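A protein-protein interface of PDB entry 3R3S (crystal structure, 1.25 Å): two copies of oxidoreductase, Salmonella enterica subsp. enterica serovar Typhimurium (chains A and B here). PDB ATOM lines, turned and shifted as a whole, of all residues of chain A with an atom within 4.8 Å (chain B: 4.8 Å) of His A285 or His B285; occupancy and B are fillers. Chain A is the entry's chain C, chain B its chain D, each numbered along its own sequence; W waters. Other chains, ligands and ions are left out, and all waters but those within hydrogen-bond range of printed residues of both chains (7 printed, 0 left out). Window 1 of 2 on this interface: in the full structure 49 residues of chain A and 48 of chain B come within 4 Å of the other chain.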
ATOM      1  N   ASN A 225      -2.967   6.751  25.394  1.00  0.00           N
ATOM      2  CA  ASN A 225      -3.421   6.079  24.181  1.00  0.00           C
ATOM      3  C   ASN A 225      -4.673   5.265  24.482  1.00  0.00           C
ATOM      4  O   ASN A 225      -5.030   5.099  25.664  1.00  0.00           O
ATOM      5  CB  ASN A 225      -2.332   5.185  23.600  1.00  0.00           C
ATOM      6  CG  ASN A 225      -1.174   5.988  23.053  1.00  0.00           C
ATOM      7  OD1 ASN A 225      -1.287   6.627  21.996  1.00  0.00           O
ATOM      8  ND2 ASN A 225      -0.060   5.987  23.774  1.00  0.00           N
ATOM      9  N   ILE A 226      -5.327   4.784  23.426  1.00  0.00           N
ATOM     10  CA  ILE A 226      -6.647   4.159  23.563  1.00  0.00           C
ATOM     11  C   ILE A 226      -6.657   2.800  22.862  1.00  0.00           C
ATOM     12  O   ILE A 226      -6.046   2.644  21.780  1.00  0.00           O
ATOM     13  CB  ILE A 226      -7.722   5.050  22.897  1.00  0.00           C
ATOM     14  CG1 ILE A 226      -7.571   6.517  23.348  1.00  0.00           C
ATOM     15  CG2 ILE A 226      -9.118   4.502  23.243  1.00  0.00           C
ATOM     16  CD1 ILE A 226      -6.800   7.437  22.371  1.00  0.00           C
ATOM     17  N   VAL A 227      -7.310   1.816  23.491  1.00  0.00           N
ATOM     18  CA  VAL A 227      -7.534   0.509  22.872  1.00  0.00           C
ATOM     19  C   VAL A 227      -9.035   0.417  22.615  1.00  0.00           C
ATOM     20  O   VAL A 227      -9.838   0.721  23.512  1.00  0.00           O
ATOM     21  CB  VAL A 227      -7.027  -0.623  23.775  1.00  0.00           C
ATOM     22  CG1 VAL A 227      -7.366  -1.975  23.129  1.00  0.00           C
ATOM     23  CG2 VAL A 227      -5.512  -0.512  23.980  1.00  0.00           C
ATOM     24  N   ALA A 228      -9.408   0.040  21.389  1.00  0.00           N
ATOM     25  CA  ALA A 228     -10.829  -0.085  21.022  1.00  0.00           C
ATOM     26  C   ALA A 228     -11.083  -1.494  20.522  1.00  0.00           C
ATOM     27  O   ALA A 228     -10.850  -1.795  19.347  1.00  0.00           O
ATOM     28  CB  ALA A 228     -11.181   0.977  19.945  1.00  0.00           C
ATOM     29  N   VAL A 268      -1.458  -5.487  22.809  1.00  0.00           N
ATOM     30  CA  VAL A 268      -1.495  -4.037  22.535  1.00  0.00           C
ATOM     31  C   VAL A 268      -1.421  -3.243  23.839  1.00  0.00           C
ATOM     32  O   VAL A 268      -0.799  -2.171  23.884  1.00  0.00           O
ATOM     33  CB  VAL A 268      -2.695  -3.633  21.641  1.00  0.00           C
ATOM     34  CG1 VAL A 268      -4.020  -3.723  22.383  1.00  0.00           C
ATOM     35  CG2 VAL A 268      -2.478  -2.211  21.087  1.00  0.00           C
ATOM     36  N   TYR A 271       2.342  -3.201  24.453  1.00  0.00           N
ATOM     37  CA  TYR A 271       2.983  -2.286  23.513  1.00  0.00           C
ATOM     38  C   TYR A 271       2.826  -0.831  23.968  1.00  0.00           C
ATOM     39  O   TYR A 271       3.798  -0.081  23.965  1.00  0.00           O
ATOM     40  CB  TYR A 271       2.355  -2.494  22.148  1.00  0.00           C
ATOM     41  CG  TYR A 271       2.576  -1.405  21.094  1.00  0.00           C
ATOM     42  CD1 TYR A 271       3.834  -1.142  20.552  1.00  0.00           C
ATOM     43  CD2 TYR A 271       1.497  -0.648  20.642  1.00  0.00           C
ATOM     44  CE1 TYR A 271       4.009  -0.170  19.568  1.00  0.00           C
ATOM     45  CE2 TYR A 271       1.661   0.335  19.652  1.00  0.00           C
ATOM     46  CZ  TYR A 271       2.925   0.579  19.134  1.00  0.00           C
ATOM     47  OH  TYR A 271       3.135   1.540  18.156  1.00  0.00           O
ATOM     48  N   LEU A 272       1.603  -0.433  24.367  1.00  0.00           N
ATOM     49  CA  LEU A 272       1.345   0.948  24.760  1.00  0.00           C
ATOM     50  C   LEU A 272       1.930   1.302  26.123  1.00  0.00           C
ATOM     51  O   LEU A 272       2.421   2.432  26.318  1.00  0.00           O
ATOM     52  CB  LEU A 272      -0.152   1.229  24.705  1.00  0.00           C
ATOM     53  CG  LEU A 272      -0.748   1.148  23.295  1.00  0.00           C
ATOM     54  CD1 LEU A 272      -2.281   1.217  23.357  1.00  0.00           C
ATOM     55  CD2 LEU A 272      -0.191   2.235  22.373  1.00  0.00           C
ATOM     56  N   VAL A 280       4.259   7.266  20.288  1.00  0.00           N
ATOM     57  CA  VAL A 280       2.819   6.970  20.196  1.00  0.00           C
ATOM     58  C   VAL A 280       2.095   7.648  21.331  1.00  0.00           C
ATOM     59  O   VAL A 280       2.256   7.283  22.516  1.00  0.00           O
ATOM     60  CB  VAL A 280       2.530   5.478  20.224  1.00  0.00           C
ATOM     61  CG1 VAL A 280       1.051   5.207  19.939  1.00  0.00           C
ATOM     62  CG2 VAL A 280       3.438   4.719  19.226  1.00  0.00           C
ATOM     63  N   GLU A 283      -3.306   8.005  20.193  1.00  0.00           N
ATOM     64  CA  GLU A 283      -3.708   7.084  19.126  1.00  0.00           C
ATOM     65  C   GLU A 283      -4.610   5.962  19.629  1.00  0.00           C
ATOM     66  O   GLU A 283      -4.436   5.478  20.739  1.00  0.00           O
ATOM     67  CB  GLU A 283      -2.482   6.449  18.474  1.00  0.00           C
ATOM     68  CG  GLU A 283      -1.515   7.450  17.809  1.00  0.00           C
ATOM     69  CD  GLU A 283      -1.977   8.129  16.516  1.00  0.00           C
ATOM     70  OE1 GLU A 283      -3.112   7.926  16.018  1.00  0.00           O
ATOM     71  OE2 GLU A 283      -1.153   8.894  15.979  1.00  0.00           O
ATOM     72  N   VAL A 284      -5.546   5.546  18.786  1.00  0.00           N
ATOM     73  CA  VAL A 284      -6.453   4.444  19.107  1.00  0.00           C
ATOM     74  C   VAL A 284      -6.048   3.196  18.335  1.00  0.00           C
ATOM     75  O   VAL A 284      -5.609   3.269  17.179  1.00  0.00           O
ATOM     76  CB  VAL A 284      -7.948   4.836  18.845  1.00  0.00           C
ATOM     77  CG1 VAL A 284      -8.222   5.077  17.340  1.00  0.00           C
ATOM     78  CG2 VAL A 284      -8.898   3.775  19.410  1.00  0.00           C
ATOM     79  N   HIS A 285      -6.194   2.052  18.987  1.00  0.00           N
ATOM     80  CA  HIS A 285      -5.720   0.779  18.443  1.00  0.00           C
ATOM     81  C   HIS A 285      -6.855  -0.203  18.463  1.00  0.00           C
ATOM     82  O   HIS A 285      -7.371  -0.570  19.535  1.00  0.00           O
ATOM     83  CB  HIS A 285      -4.545   0.235  19.275  1.00  0.00           C
ATOM     84  CG  HIS A 285      -3.405   1.202  19.339  1.00  0.00           C
ATOM     85  ND1 HIS A 285      -3.445   2.387  20.050  1.00  0.00           N
ATOM     86  CD2 HIS A 285      -2.208   1.185  18.709  1.00  0.00           C
ATOM     87  CE1 HIS A 285      -2.331   3.072  19.822  1.00  0.00           C
ATOM     88  NE2 HIS A 285      -1.561   2.358  19.020  1.00  0.00           N
ATOM     89  N   GLY A 286      -7.247  -0.658  17.285  1.00  0.00           N
ATOM     90  CA  GLY A 286      -8.348  -1.607  17.154  1.00  0.00           C
ATOM     91  C   GLY A 286      -7.908  -3.056  17.261  1.00  0.00           C
ATOM     92  O   GLY A 286      -6.851  -3.445  16.737  1.00  0.00           O
ATOM     93  N   VAL A 287      -8.735  -3.863  17.932  1.00  0.00           N
ATOM     94  CA  VAL A 287      -8.533  -5.326  18.038  1.00  0.00           C
ATOM     95  C   VAL A 287      -9.941  -5.905  17.847  1.00  0.00           C
ATOM     96  O   VAL A 287     -10.661  -6.136  18.808  1.00  0.00           O
ATOM     97  CB  VAL A 287      -7.883  -5.722  19.386  1.00  0.00           C
ATOM     98  CG1 VAL A 287      -7.610  -7.230  19.411  1.00  0.00           C
ATOM     99  CG2 VAL A 287      -6.589  -4.900  19.631  1.00  0.00           C
ATOM    100  N   LEU A 293     -12.037  -0.189  12.961  1.00  0.00           N
ATOM    101  CA  LEU A 293     -12.297   1.189  13.345  1.00  0.00           C
ATOM    102  C   LEU A 293     -12.225   2.074  12.095  1.00  0.00           C
ATOM    103  O   LEU A 293     -11.848   1.649  11.030  1.00  0.00           O
ATOM    104  CB  LEU A 293     -11.231   1.686  14.339  1.00  0.00           C
ATOM    105  CG  LEU A 293     -10.915   0.788  15.547  1.00  0.00           C
ATOM    106  CD1 LEU A 293      -9.851   1.472  16.431  1.00  0.00           C
ATOM    107  CD2 LEU A 293     -12.187   0.495  16.377  1.00  0.00           C
ATOM    108  N   ASN B 225      -2.678  -5.438   7.921  1.00  0.00           N
ATOM    109  CA  ASN B 225      -2.813  -4.258   8.772  1.00  0.00           C
ATOM    110  C   ASN B 225      -1.947  -3.150   8.232  1.00  0.00           C
ATOM    111  O   ASN B 225      -1.102  -3.383   7.349  1.00  0.00           O
ATOM    112  CB  ASN B 225      -2.456  -4.568  10.234  1.00  0.00           C
ATOM    113  CG  ASN B 225      -3.452  -5.496  10.881  1.00  0.00           C
ATOM    114  OD1 ASN B 225      -4.581  -5.095  11.195  1.00  0.00           O
ATOM    115  ND2 ASN B 225      -3.056  -6.760  11.057  1.00  0.00           N
ATOM    116  N   ILE B 226      -2.141  -1.944   8.779  1.00  0.00           N
ATOM    117  CA  ILE B 226      -1.520  -0.738   8.227  1.00  0.00           C
ATOM    118  C   ILE B 226      -0.829   0.037   9.333  1.00  0.00           C
ATOM    119  O   ILE B 226      -1.368   0.138  10.453  1.00  0.00           O
ATOM    120  CB  ILE B 226      -2.607   0.181   7.577  1.00  0.00           C
ATOM    121  CG1 ILE B 226      -3.563  -0.610   6.651  1.00  0.00           C
ATOM    122  CG2 ILE B 226      -1.936   1.320   6.832  1.00  0.00           C
ATOM    123  CD1 ILE B 226      -4.868  -1.074   7.332  1.00  0.00           C
ATOM    124  N   VAL B 227       0.370   0.549   9.032  1.00  0.00           N
ATOM    125  CA  VAL B 227       1.059   1.470   9.929  1.00  0.00           C
ATOM    126  C   VAL B 227       1.029   2.840   9.256  1.00  0.00           C
ATOM    127  O   VAL B 227       1.353   2.974   8.070  1.00  0.00           O
ATOM    128  CB  VAL B 227       2.521   1.006  10.187  1.00  0.00           C
ATOM    129  CG1 VAL B 227       3.283   2.037  11.027  1.00  0.00           C
ATOM    130  CG2 VAL B 227       2.491  -0.354  10.872  1.00  0.00           C
ATOM    131  N   ALA B 228       0.638   3.866  10.007  1.00  0.00           N
ATOM    132  CA  ALA B 228       0.556   5.249   9.482  1.00  0.00           C
ATOM    133  C   ALA B 228       1.439   6.143  10.349  1.00  0.00           C
ATOM    134  O   ALA B 228       1.006   6.632  11.385  1.00  0.00           O
ATOM    135  CB  ALA B 228      -0.910   5.735   9.471  1.00  0.00           C
ATOM    136  N   VAL B 268       5.758  -1.406  16.400  1.00  0.00           N
ATOM    137  CA  VAL B 268       4.447  -1.747  15.853  1.00  0.00           C
ATOM    138  C   VAL B 268       4.557  -2.722  14.680  1.00  0.00           C
ATOM    139  O   VAL B 268       3.680  -3.559  14.491  1.00  0.00           O
ATOM    140  CB  VAL B 268       3.621  -0.481  15.516  1.00  0.00           C
ATOM    141  CG1 VAL B 268       4.168   0.250  14.256  1.00  0.00           C
ATOM    142  CG2 VAL B 268       2.159  -0.826  15.361  1.00  0.00           C
ATOM    143  N   TYR B 271       4.767  -6.049  16.450  1.00  0.00           N
ATOM    144  CA  TYR B 271       3.455  -6.392  17.007  1.00  0.00           C
ATOM    145  C   TYR B 271       2.544  -6.981  15.928  1.00  0.00           C
ATOM    146  O   TYR B 271       1.925  -8.034  16.126  1.00  0.00           O
ATOM    147  CB  TYR B 271       2.850  -5.160  17.673  1.00  0.00           C
ATOM    148  CG  TYR B 271       1.343  -5.182  17.926  1.00  0.00           C
ATOM    149  CD1 TYR B 271       0.787  -6.048  18.850  1.00  0.00           C
ATOM    150  CD2 TYR B 271       0.502  -4.320  17.221  1.00  0.00           C
ATOM    151  CE1 TYR B 271      -0.584  -6.035  19.106  1.00  0.00           C
ATOM    152  CE2 TYR B 271      -0.879  -4.293  17.471  1.00  0.00           C
ATOM    153  CZ  TYR B 271      -1.405  -5.179  18.380  1.00  0.00           C
ATOM    154  OH  TYR B 271      -2.750  -5.181  18.660  1.00  0.00           O
ATOM    155  N   LEU B 272       2.492  -6.326  14.767  1.00  0.00           N
ATOM    156  CA  LEU B 272       1.584  -6.730  13.690  1.00  0.00           C
ATOM    157  C   LEU B 272       2.080  -7.997  12.976  1.00  0.00           C
ATOM    158  O   LEU B 272       1.272  -8.835  12.566  1.00  0.00           O
ATOM    159  CB  LEU B 272       1.416  -5.573  12.689  1.00  0.00           C
ATOM    160  CG  LEU B 272       0.636  -4.394  13.306  1.00  0.00           C
ATOM    161  CD1 LEU B 272       0.618  -3.230  12.345  1.00  0.00           C
ATOM    162  CD2 LEU B 272      -0.774  -4.806  13.734  1.00  0.00           C
ATOM    163  N   VAL B 280      -6.221  -8.990  15.207  1.00  0.00           N
ATOM    164  CA  VAL B 280      -6.015  -7.694  14.564  1.00  0.00           C
ATOM    165  C   VAL B 280      -5.888  -7.884  13.054  1.00  0.00           C
ATOM    166  O   VAL B 280      -4.897  -8.451  12.557  1.00  0.00           O
ATOM    167  CB  VAL B 280      -4.762  -6.957  15.123  1.00  0.00           C
ATOM    168  CG1 VAL B 280      -4.661  -5.530  14.566  1.00  0.00           C
ATOM    169  CG2 VAL B 280      -4.776  -6.981  16.653  1.00  0.00           C
ATOM    170  N   GLU B 283      -6.692  -3.072  10.496  1.00  0.00           N
ATOM    171  CA  GLU B 283      -6.554  -1.913  11.409  1.00  0.00           C
ATOM    172  C   GLU B 283      -5.320  -1.061  11.093  1.00  0.00           C
ATOM    173  O   GLU B 283      -4.277  -1.593  10.684  1.00  0.00           O
ATOM    174  CB  GLU B 283      -6.447  -2.380  12.876  1.00  0.00           C
ATOM    175  CG  GLU B 283      -7.654  -3.164  13.364  1.00  0.00           C
ATOM    176  CD  GLU B 283      -8.967  -2.383  13.558  1.00  0.00           C
ATOM    177  OE1 GLU B 283      -9.065  -1.154  13.324  1.00  0.00           O
ATOM    178  OE2 GLU B 283      -9.931  -3.045  14.021  1.00  0.00           O
ATOM    179  N   VAL B 284      -5.441   0.244  11.295  1.00  0.00           N
ATOM    180  CA  VAL B 284      -4.356   1.177  11.067  1.00  0.00           C
ATOM    181  C   VAL B 284      -3.798   1.642  12.420  1.00  0.00           C
ATOM    182  O   VAL B 284      -4.532   1.813  13.395  1.00  0.00           O
ATOM    183  CB  VAL B 284      -4.796   2.395  10.195  1.00  0.00           C
ATOM    184  CG1 VAL B 284      -5.882   3.260  10.880  1.00  0.00           C
ATOM    185  CG2 VAL B 284      -3.586   3.265   9.830  1.00  0.00           C
ATOM    186  N   HIS B 285      -2.477   1.791  12.465  1.00  0.00           N
ATOM    187  CA  HIS B 285      -1.762   2.117  13.694  1.00  0.00           C
ATOM    188  C   HIS B 285      -0.920   3.355  13.506  1.00  0.00           C
ATOM    189  O   HIS B 285      -0.011   3.377  12.696  1.00  0.00           O
ATOM    190  CB  HIS B 285      -0.879   0.914  14.058  1.00  0.00           C
ATOM    191  CG  HIS B 285      -1.672  -0.341  14.266  1.00  0.00           C
ATOM    192  ND1 HIS B 285      -2.218  -1.054  13.223  1.00  0.00           N
ATOM    193  CD2 HIS B 285      -2.044  -0.981  15.399  1.00  0.00           C
ATOM    194  CE1 HIS B 285      -2.909  -2.075  13.705  1.00  0.00           C
ATOM    195  NE2 HIS B 285      -2.811  -2.057  15.020  1.00  0.00           N
ATOM    196  N   GLY B 286      -1.227   4.373  14.281  1.00  0.00           N
ATOM    197  CA  GLY B 286      -0.515   5.639  14.207  1.00  0.00           C
ATOM    198  C   GLY B 286       0.704   5.705  15.107  1.00  0.00           C
ATOM    199  O   GLY B 286       0.699   5.222  16.237  1.00  0.00           O
ATOM    200  N   VAL B 287       1.772   6.303  14.564  1.00  0.00           N
ATOM    201  CA  VAL B 287       3.014   6.554  15.323  1.00  0.00           C
ATOM    202  C   VAL B 287       3.407   7.980  14.917  1.00  0.00           C
ATOM    203  O   VAL B 287       4.207   8.168  14.001  1.00  0.00           O
ATOM    204  CB  VAL B 287       4.097   5.513  14.991  1.00  0.00           C
ATOM    205  CG1 VAL B 287       5.301   5.744  15.897  1.00  0.00           C
ATOM    206  CG2 VAL B 287       3.539   4.065  15.176  1.00  0.00           C
ATOM    207  N   LEU B 293      -4.033  10.135  14.057  1.00  0.00           N
ATOM    208  CA  LEU B 293      -4.931   9.737  12.984  1.00  0.00           C
ATOM    209  C   LEU B 293      -6.385  10.039  13.380  1.00  0.00           C
ATOM    210  O   LEU B 293      -6.687  10.366  14.539  1.00  0.00           O
ATOM    211  CB  LEU B 293      -4.822   8.226  12.735  1.00  0.00           C
ATOM    212  CG  LEU B 293      -3.378   7.697  12.539  1.00  0.00           C
ATOM    213  CD1 LEU B 293      -3.468   6.165  12.258  1.00  0.00           C
ATOM    214  CD2 LEU B 293      -2.603   8.434  11.424  1.00  0.00           C
HETATM  215  O   HOH W   1       0.736   2.593  17.266  1.00  0.00           O
HETATM  216  O   HOH W   2       6.002   1.471  17.112  1.00  0.00           O
HETATM  217  O   HOH W   3      -4.085  -3.175  17.361  1.00  0.00           O
HETATM  218  O   HOH W   4      -3.393  -6.924  21.066  1.00  0.00           O
HETATM  219  O   HOH W   5      -3.720   4.608  15.487  1.00  0.00           O
HETATM  220  O   HOH W   6      -6.806   2.922  14.507  1.00  0.00           O
HETATM  221  O   HOH W   7      -5.309  -0.175  15.295  1.00  0.00           O
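Of the 14 printed residues of chain B, 8 touch a printed residue of chain A. Printed residues of chain B that touch a printed residue of chain A: Val B268, Tyr B271, Val B280, Glu B283, His B285, Gly B286, Val B287 and Leu B293. Of the 14 printed residues of chain A, 8 touch a printed residue of chain B. Printed residues of chain A that touch a printed residue of chain B: Val A268, Tyr A271, Val A280, Glu A283, His A285, Gly A286, Val A287 and Leu A293. Along chain A the printed residues that touch a printed residue of chain B span positions 268 to 293. Among the printed residues, 13 pairs touch across the chains.
Tyr A271 touches Val B287, and with the chains exchanged Val A287 touches Tyr B271. Val A280 touches Gly B286, and with the chains exchanged Gly A286 touches Val B280. Val A280 touches Val B287, and with the chains exchanged Val A287 touches Val B280. His B285 touches its own counterpart, His A285.
N of Leu B293 sits at hydrogen-bond distance from OE1 of Glu A283 (3.1 Å). The side-chain carboxylate (OE1) of Glu B283 is in hydrogen-bond range of the backbone NH (N) of Leu A293 (3.1 Å).
Of chain B, only His B285 (3.96 Å) comes within 4 Å of His A285. Printed residues of chain B within 4 Å of Gly A286: Val B280 (3.7 Å) and Glu B283 (3.5 Å). Of the printed residues of chain B, Val A287 touches Tyr B271 and Val B280. Of the printed residues of chain A, Glu B283 touches Gly A286 and Leu A293. His B285 touches just one residue of chain A: His A285. Printed residues of chain A within 4 Å of Gly B286: Val A280 and Glu A283. Of the printed residues of chain A, Leu B293 touches Glu A283. The nearest residue of chain A that does not touch His B285 is Gly A286 (4.6 Å). The nearest printed residue of chain A that does not touch Tyr B271 is Gly A286 (4.9 Å).
Water W3 lies within hydrogen-bond range of OH of Tyr B271, O of Gly A286 and NE2 of His B285. Water W6 lies within hydrogen-bond range of the backbone carbonyl oxygen (O) of Val B284 (2.8 Å) and the backbone carbonyl oxygen (O) of Val A284 (2.9 Å). Water W5 lies within hydrogen-bond range of the backbone NH of Gly B286 (2.8 Å), the backbone carbonyl oxygen of Val A284 (2.9 Å) and the side-chain carboxylate of Glu A283 (3.4 Å). Water W7 lies within hydrogen-bond range of the backbone NH (N) of Gly A286, the backbone carbonyl oxygen (O) of Val B284 and a ring nitrogen (NE2) of His B285. Water W2 bridges N of Val B268 and OH of Tyr A271. Water W4 lies within hydrogen-bond range of the backbone NH (N) of Val A268 and the side-chain hydroxyl (OH) of Tyr B271.
Among the printed residues, merely in contact across the chains: Val A268 with Tyr B271, Tyr A271 with Val B268, Gly A286 with Glu B283, Glu A283 with Gly B286, Val A280 with Gly B286, Gly A286 with Val B280, Tyr A271 with Val B287, Val A280 with Val B287, His A285 with His B285, Val A287 with Val B280 and Val A287 with Tyr B271.
The backbone carbonyl oxygen (O) of Ile A226 lies within hydrogen-bond range of the backbone NH (N) of His A285 (2.9 Å). The backbone NH (N) of Ile B226 lies within hydrogen-bond range of the backbone carbonyl oxygen (O) of Glu B283, at 2.9 Å. N of Glu B283 lies within hydrogen-bond range of OD1 of Asn B225, 3.0 Å away. OD1 of Asn A225 sits at hydrogen-bond distance from N of Glu A283 (3.0 Å). The side-chain amide nitrogen (ND2) of Asn B225 lies within hydrogen-bond range of the backbone carbonyl oxygen (O) of Val B280. The backbone NH (N) of His B285 lies within hydrogen-bond range of the backbone carbonyl oxygen (O) of Ile B226 (2.8 Å).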
